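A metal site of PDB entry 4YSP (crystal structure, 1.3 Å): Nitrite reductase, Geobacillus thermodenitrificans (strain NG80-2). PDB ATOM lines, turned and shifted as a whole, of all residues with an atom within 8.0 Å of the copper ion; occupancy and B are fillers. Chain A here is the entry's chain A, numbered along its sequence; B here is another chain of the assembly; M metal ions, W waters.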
ATOM      1  N   ASP A  98      19.727  -6.680 -16.080  1.00  0.00           N
ATOM      2  CA  ASP A  98      18.931  -7.406 -17.057  1.00  0.00           C
ATOM      3  C   ASP A  98      19.928  -8.040 -17.987  1.00  0.00           C
ATOM      4  O   ASP A  98      20.684  -7.369 -18.684  1.00  0.00           O
ATOM      5  CB  ASP A  98      18.084  -6.449 -17.835  1.00  0.00           C
ATOM      6  CG  ASP A  98      17.290  -7.052 -19.017  1.00  0.00           C
ATOM      7  OD1 ASP A  98      17.700  -8.104 -19.528  1.00  0.00           O
ATOM      8  OD2 ASP A  98      16.263  -6.413 -19.381  1.00  0.00           O
ATOM      9  N   PHE A  99      19.963  -9.419 -18.039  1.00  0.00           N
ATOM     10  CA  PHE A  99      20.733 -10.134 -19.047  1.00  0.00           C
ATOM     11  C   PHE A  99      19.794 -10.544 -20.168  1.00  0.00           C
ATOM     12  O   PHE A  99      18.838 -11.272 -19.891  1.00  0.00           O
ATOM     13  CB  PHE A  99      21.341 -11.394 -18.485  1.00  0.00           C
ATOM     14  CG  PHE A  99      22.475 -11.171 -17.490  1.00  0.00           C
ATOM     15  CD1 PHE A  99      23.743 -10.906 -17.909  1.00  0.00           C
ATOM     16  CD2 PHE A  99      22.293 -11.403 -16.145  1.00  0.00           C
ATOM     17  CE1 PHE A  99      24.792 -10.726 -16.985  1.00  0.00           C
ATOM     18  CE2 PHE A  99      23.323 -11.254 -15.260  1.00  0.00           C
ATOM     19  CZ  PHE A  99      24.551 -10.909 -15.666  1.00  0.00           C
ATOM     20  N   HIS A 100      20.017 -10.143 -21.409  1.00  0.00           N
ATOM     21  CA  HIS A 100      19.171 -10.589 -22.474  1.00  0.00           C
ATOM     22  C   HIS A 100      19.268 -12.092 -22.732  1.00  0.00           C
ATOM     23  O   HIS A 100      18.430 -12.696 -23.371  1.00  0.00           O
ATOM     24  CB  HIS A 100      19.496  -9.909 -23.803  1.00  0.00           C
ATOM     25  CG  HIS A 100      18.993  -8.504 -23.877  1.00  0.00           C
ATOM     26  ND1 HIS A 100      18.941  -7.864 -25.071  1.00  0.00           N
ATOM     27  CD2 HIS A 100      18.474  -7.665 -22.961  1.00  0.00           C
ATOM     28  CE1 HIS A 100      18.431  -6.657 -24.848  1.00  0.00           C
ATOM     29  NE2 HIS A 100      18.136  -6.523 -23.599  1.00  0.00           N
ATOM     30  N   PHE A 110      14.923  -8.831 -12.089  1.00  0.00           N
ATOM     31  CA  PHE A 110      15.704  -7.698 -12.616  1.00  0.00           C
ATOM     32  C   PHE A 110      15.404  -6.447 -11.793  1.00  0.00           C
ATOM     33  O   PHE A 110      15.431  -5.376 -12.283  1.00  0.00           O
ATOM     34  CB  PHE A 110      15.377  -7.413 -14.111  1.00  0.00           C
ATOM     35  CG  PHE A 110      15.674  -8.550 -15.099  1.00  0.00           C
ATOM     36  CD1 PHE A 110      16.492  -9.604 -14.796  1.00  0.00           C
ATOM     37  CD2 PHE A 110      15.160  -8.459 -16.389  1.00  0.00           C
ATOM     38  CE1 PHE A 110      16.781 -10.575 -15.747  1.00  0.00           C
ATOM     39  CE2 PHE A 110      15.441  -9.415 -17.317  1.00  0.00           C
ATOM     40  CZ  PHE A 110      16.247 -10.470 -17.009  1.00  0.00           C
ATOM     41  N   MET A 132      23.109  -8.651 -25.200  1.00  0.00           N
ATOM     42  CA  MET A 132      23.311  -7.504 -24.355  1.00  0.00           C
ATOM     43  C   MET A 132      22.942  -7.784 -22.892  1.00  0.00           C
ATOM     44  O   MET A 132      21.977  -8.531 -22.624  1.00  0.00           O
ATOM     45  CB  MET A 132      22.491  -6.349 -24.859  1.00  0.00           C
ATOM     46  CG  MET A 132      22.599  -5.024 -24.103  1.00  0.00           C
ATOM     47  SD  MET A 132      21.770  -3.709 -24.954  1.00  0.00           S
ATOM     48  CE  MET A 132      22.009  -2.325 -23.820  1.00  0.00           C
ATOM     49  N   TYR A 133      23.637  -7.143 -21.982  1.00  0.00           N
ATOM     50  CA  TYR A 133      23.167  -6.958 -20.642  1.00  0.00           C
ATOM     51  C   TYR A 133      23.169  -5.454 -20.307  1.00  0.00           C
ATOM     52  O   TYR A 133      23.907  -4.712 -20.915  1.00  0.00           O
ATOM     53  CB  TYR A 133      23.921  -7.788 -19.583  1.00  0.00           C
ATOM     54  CG  TYR A 133      25.331  -7.374 -19.237  1.00  0.00           C
ATOM     55  CD1 TYR A 133      25.595  -6.235 -18.489  1.00  0.00           C
ATOM     56  CD2 TYR A 133      26.396  -8.137 -19.617  1.00  0.00           C
ATOM     57  CE1 TYR A 133      26.895  -5.890 -18.110  1.00  0.00           C
ATOM     58  CE2 TYR A 133      27.723  -7.854 -19.240  1.00  0.00           C
ATOM     59  CZ  TYR A 133      27.955  -6.742 -18.502  1.00  0.00           C
ATOM     60  OH  TYR A 133      29.203  -6.315 -18.080  1.00  0.00           O
ATOM     61  N   HIS A 134      22.366  -5.044 -19.355  1.00  0.00           N
ATOM     62  CA  HIS A 134      22.294  -3.649 -18.955  1.00  0.00           C
ATOM     63  C   HIS A 134      21.540  -3.478 -17.669  1.00  0.00           C
ATOM     64  O   HIS A 134      20.796  -4.344 -17.262  1.00  0.00           O
ATOM     65  CB  HIS A 134      21.713  -2.809 -20.058  1.00  0.00           C
ATOM     66  CG  HIS A 134      20.303  -3.169 -20.413  1.00  0.00           C
ATOM     67  ND1 HIS A 134      19.198  -2.725 -19.747  1.00  0.00           N
ATOM     68  CD2 HIS A 134      19.830  -4.018 -21.364  1.00  0.00           C
ATOM     69  CE1 HIS A 134      18.095  -3.228 -20.324  1.00  0.00           C
ATOM     70  NE2 HIS A 134      18.462  -4.002 -21.326  1.00  0.00           N
ATOM     71  N   CYS A 135      21.730  -2.325 -17.052  1.00  0.00           N
ATOM     72  CA  CYS A 135      20.892  -1.949 -15.922  1.00  0.00           C
ATOM     73  C   CYS A 135      19.474  -1.802 -16.404  1.00  0.00           C
ATOM     74  O   CYS A 135      19.231  -1.184 -17.464  1.00  0.00           O
ATOM     75  CB  CYS A 135      21.446  -0.692 -15.285  1.00  0.00           C
ATOM     76  SG  CYS A 135      20.496  -0.138 -13.869  1.00  0.00           S
ATOM     77  N   GLY A 136      18.515  -2.198 -15.563  1.00  0.00           N
ATOM     78  CA  GLY A 136      17.103  -2.131 -15.848  1.00  0.00           C
ATOM     79  C   GLY A 136      16.301  -1.171 -14.952  1.00  0.00           C
ATOM     80  O   GLY A 136      15.129  -1.313 -14.831  1.00  0.00           O
ATOM     81  N   VAL A 140      15.295   3.593 -17.837  1.00  0.00           N
ATOM     82  CA  VAL A 140      16.299   2.709 -18.388  1.00  0.00           C
ATOM     83  C   VAL A 140      17.198   3.426 -19.357  1.00  0.00           C
ATOM     84  O   VAL A 140      18.431   3.240 -19.328  1.00  0.00           O
ATOM     85  CB  VAL A 140      15.680   1.406 -18.964  1.00  0.00           C
ATOM     86  CG1 VAL A 140      16.714   0.590 -19.619  1.00  0.00           C
ATOM     87  CG2 VAL A 140      14.964   0.620 -17.850  1.00  0.00           C
ATOM     88  N   ILE A 144      21.329   3.148 -19.131  1.00  0.00           N
ATOM     89  CA  ILE A 144      22.093   2.646 -20.247  1.00  0.00           C
ATOM     90  C   ILE A 144      22.977   3.761 -20.788  1.00  0.00           C
ATOM     91  O   ILE A 144      24.209   3.584 -20.960  1.00  0.00           O
ATOM     92  CB  ILE A 144      21.218   2.048 -21.363  1.00  0.00           C
ATOM     93  CG1 ILE A 144      20.413   0.876 -20.845  1.00  0.00           C
ATOM     94  CG2 ILE A 144      22.089   1.655 -22.549  1.00  0.00           C
ATOM     95  CD1 ILE A 144      19.469   0.256 -21.907  1.00  0.00           C
ATOM     96  N   VAL A 235      25.156  -2.118 -28.329  1.00  0.00           N
ATOM     97  CA  VAL A 235      24.351  -1.847 -27.153  1.00  0.00           C
ATOM     98  C   VAL A 235      23.563  -0.592 -27.191  1.00  0.00           C
ATOM     99  O   VAL A 235      22.707  -0.328 -26.310  1.00  0.00           O
ATOM    100  CB  VAL A 235      25.130  -1.999 -25.837  1.00  0.00           C
ATOM    101  CG1 VAL A 235      25.716  -3.395 -25.723  1.00  0.00           C
ATOM    102  CG2 VAL A 235      26.186  -0.947 -25.720  1.00  0.00           C
ATOM    103  N   ALA A 273      19.516  -1.893 -32.152  1.00  0.00           N
ATOM    104  CA  ALA A 273      19.990  -1.612 -30.823  1.00  0.00           C
ATOM    105  C   ALA A 273      19.741  -2.837 -29.954  1.00  0.00           C
ATOM    106  O   ALA A 273      18.597  -3.367 -29.927  1.00  0.00           O
ATOM    107  CB  ALA A 273      19.229  -0.403 -30.263  1.00  0.00           C
ATOM    108  N   SER A 274      20.788  -3.267 -29.270  1.00  0.00           N
ATOM    109  CA  SER A 274      20.912  -4.521 -28.465  1.00  0.00           C
ATOM    110  C   SER A 274      21.246  -5.722 -29.328  1.00  0.00           C
ATOM    111  O   SER A 274      21.399  -6.768 -28.818  1.00  0.00           O
ATOM    112  CB  SER A 274      19.738  -4.805 -27.525  1.00  0.00           C
ATOM    113  OG  SER A 274      18.672  -5.353 -28.254  1.00  0.00           O
ATOM    114  N   HIS B 244      12.014  -5.993 -28.780  1.00  0.00           N
ATOM    115  CA  HIS B 244      12.491  -6.877 -27.701  1.00  0.00           C
ATOM    116  C   HIS B 244      11.464  -7.090 -26.599  1.00  0.00           C
ATOM    117  O   HIS B 244      10.836  -6.203 -26.159  1.00  0.00           O
ATOM    118  CB  HIS B 244      13.737  -6.217 -27.055  1.00  0.00           C
ATOM    119  CG  HIS B 244      14.367  -6.996 -25.948  1.00  0.00           C
ATOM    120  ND1 HIS B 244      15.120  -8.128 -26.155  1.00  0.00           N
ATOM    121  CD2 HIS B 244      14.345  -6.791 -24.626  1.00  0.00           C
ATOM    122  CE1 HIS B 244      15.547  -8.559 -24.988  1.00  0.00           C
ATOM    123  NE2 HIS B 244      15.065  -7.788 -24.050  1.00  0.00           N
ATOM    124  N   VAL B 245      11.389  -8.309 -26.088  1.00  0.00           N
ATOM    125  CA  VAL B 245      10.590  -8.578 -24.896  1.00  0.00           C
ATOM    126  C   VAL B 245      11.563  -8.897 -23.747  1.00  0.00           C
ATOM    127  O   VAL B 245      12.381  -9.788 -23.809  1.00  0.00           O
ATOM    128  CB  VAL B 245       9.591  -9.765 -25.133  1.00  0.00           C
ATOM    129  CG1 VAL B 245       8.808 -10.049 -23.881  1.00  0.00           C
ATOM    130  CG2 VAL B 245       8.626  -9.442 -26.300  1.00  0.00           C
ATOM    131  N   VAL B 246      11.434  -8.069 -22.725  1.00  0.00           N
ATOM    132  CA  VAL B 246      12.314  -8.210 -21.540  1.00  0.00           C
ATOM    133  C   VAL B 246      12.047  -9.557 -20.844  1.00  0.00           C
ATOM    134  O   VAL B 246      10.888  -9.939 -20.664  1.00  0.00           O
ATOM    135  CB  VAL B 246      12.060  -7.081 -20.603  1.00  0.00           C
ATOM    136  CG1 VAL B 246      12.977  -7.139 -19.381  1.00  0.00           C
ATOM    137  CG2 VAL B 246      12.270  -5.751 -21.272  1.00  0.00           C
ATOM    138  N   GLY B 247      13.094 -10.267 -20.443  1.00  0.00           N
ATOM    139  CA  GLY B 247      12.970 -11.501 -19.666  1.00  0.00           C
ATOM    140  C   GLY B 247      12.762 -12.785 -20.458  1.00  0.00           C
ATOM    141  O   GLY B 247      12.574 -13.828 -19.865  1.00  0.00           O
ATOM    142  N   GLN B 267      17.392 -12.276 -29.699  1.00  0.00           N
ATOM    143  CA  GLN B 267      17.057 -11.415 -28.593  1.00  0.00           C
ATOM    144  C   GLN B 267      16.153 -10.214 -28.989  1.00  0.00           C
ATOM    145  O   GLN B 267      15.282  -9.810 -28.215  1.00  0.00           O
ATOM    146  CB  GLN B 267      18.333 -10.888 -27.875  1.00  0.00           C
ATOM    147  CG  GLN B 267      19.124  -9.826 -28.651  1.00  0.00           C
ATOM    148  CD  GLN B 267      20.492  -9.666 -27.993  1.00  0.00           C
ATOM    149  OE1 GLN B 267      20.617  -9.256 -26.835  1.00  0.00           O
ATOM    150  NE2 GLN B 267      21.494 -10.048 -28.736  1.00  0.00           N
ATOM    151  N   THR B 268      16.392  -9.706 -30.162  1.00  0.00           N
ATOM    152  CA  THR B 268      15.849  -8.468 -30.677  1.00  0.00           C
ATOM    153  C   THR B 268      15.648  -8.587 -32.170  1.00  0.00           C
ATOM    154  O   THR B 268      16.504  -9.142 -32.874  1.00  0.00           O
ATOM    155  CB  THR B 268      16.752  -7.309 -30.322  1.00  0.00           C
ATOM    156  OG1 THR B 268      16.812  -7.269 -28.879  1.00  0.00           O
ATOM    157  CG2 THR B 268      16.274  -5.992 -30.868  1.00  0.00           C
ATOM    158  N   VAL B 292       9.482  -3.686 -25.570  1.00  0.00           N
ATOM    159  CA  VAL B 292      10.072  -2.421 -25.915  1.00  0.00           C
ATOM    160  C   VAL B 292      10.527  -2.398 -27.345  1.00  0.00           C
ATOM    161  O   VAL B 292      10.747  -3.434 -27.995  1.00  0.00           O
ATOM    162  CB  VAL B 292      11.291  -2.015 -24.994  1.00  0.00           C
ATOM    163  CG1 VAL B 292      10.870  -2.105 -23.587  1.00  0.00           C
ATOM    164  CG2 VAL B 292      12.497  -2.912 -25.253  1.00  0.00           C
ATOM    165  N   THR B 293      10.721  -1.149 -27.896  1.00  0.00           N
ATOM    166  CA  THR B 293      11.781  -1.005 -28.888  1.00  0.00           C
ATOM    167  C   THR B 293      13.066  -0.653 -28.085  1.00  0.00           C
ATOM    168  O   THR B 293      13.030   0.226 -27.189  1.00  0.00           O
ATOM    169  CB  THR B 293      11.478   0.072 -29.964  1.00  0.00           C
ATOM    170  OG1 THR B 293      12.701   0.184 -30.756  1.00  0.00           O
ATOM    171  CG2 THR B 293      11.129   1.406 -29.390  1.00  0.00           C
ATOM    172  N   HIS B 294      14.136  -1.335 -28.376  1.00  0.00           N
ATOM    173  CA  HIS B 294      15.364  -1.199 -27.652  1.00  0.00           C
ATOM    174  C   HIS B 294      16.193   0.002 -28.040  1.00  0.00           C
ATOM    175  O   HIS B 294      17.268   0.245 -27.494  1.00  0.00           O
ATOM    176  CB  HIS B 294      16.206  -2.437 -27.687  1.00  0.00           C
ATOM    177  CG  HIS B 294      16.854  -2.768 -26.395  1.00  0.00           C
ATOM    178  ND1 HIS B 294      17.958  -2.124 -25.884  1.00  0.00           N
ATOM    179  CD2 HIS B 294      16.500  -3.729 -25.464  1.00  0.00           C
ATOM    180  CE1 HIS B 294      18.232  -2.659 -24.666  1.00  0.00           C
ATOM    181  NE2 HIS B 294      17.355  -3.650 -24.417  1.00  0.00           N
ATOM    182  N   PHE B 296      16.348   3.175 -27.090  1.00  0.00           N
ATOM    183  CA  PHE B 296      15.737   3.540 -25.804  1.00  0.00           C
ATOM    184  C   PHE B 296      15.252   4.994 -25.701  1.00  0.00           C
ATOM    185  O   PHE B 296      14.457   5.275 -24.856  1.00  0.00           O
ATOM    186  CB  PHE B 296      16.588   3.111 -24.580  1.00  0.00           C
ATOM    187  CG  PHE B 296      15.977   1.979 -23.863  1.00  0.00           C
ATOM    188  CD1 PHE B 296      14.990   2.168 -22.925  1.00  0.00           C
ATOM    189  CD2 PHE B 296      16.324   0.721 -24.205  1.00  0.00           C
ATOM    190  CE1 PHE B 296      14.404   1.107 -22.325  1.00  0.00           C
ATOM    191  CE2 PHE B 296      15.757  -0.361 -23.603  1.00  0.00           C
ATOM    192  CZ  PHE B 296      14.778  -0.168 -22.683  1.00  0.00           C
HETATM  193 CU    CU M   1      17.354  -4.807 -22.801  1.00  0.00          CU
HETATM  194  O   HOH W   1      15.198  -4.413 -22.218  1.00  0.00           O
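The copper ion is bound by NE2 of His 294 of chain B (2.0 Å), NE2 of His 134 (2.0 Å), NE2 of His 100 (2.0 Å) and water W1 (2.3 Å).
Asp 98 touches the copper ion (OD2 to CU, 3.9 Å). His 244 of chain B touches the copper ion. The nearest printed residue that does not touch the copper ion is Phe 296 of chain B (4.8 Å).
ND1 of His 100 is in hydrogen-bond range of OE1 of Gln 267 of chain B (2.8 Å). The backbone NH (N) of His 100 sits at hydrogen-bond distance from the backbone carbonyl oxygen (O) of Met 132 (2.8 Å). The backbone carbonyl oxygen of His 244 of chain B is in hydrogen-bond range of the backbone NH of Val 292 of chain B. A ring nitrogen (NE2) of His 100 lies close to a ring nitrogen (NE2) of His 244 of chain B (3.4 Å). The side-chain hydroxyl of Thr 268 of chain B sits at hydrogen-bond distance from a ring nitrogen (ND1) of His 244 of chain B (3.3 Å). The backbone carbonyl oxygen of Gln 267 of chain B sits at hydrogen-bond distance from a ring nitrogen (ND1) of His 244 of chain B. O of His 134 is in hydrogen-bond range of N of Asp 98 (2.8 Å).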
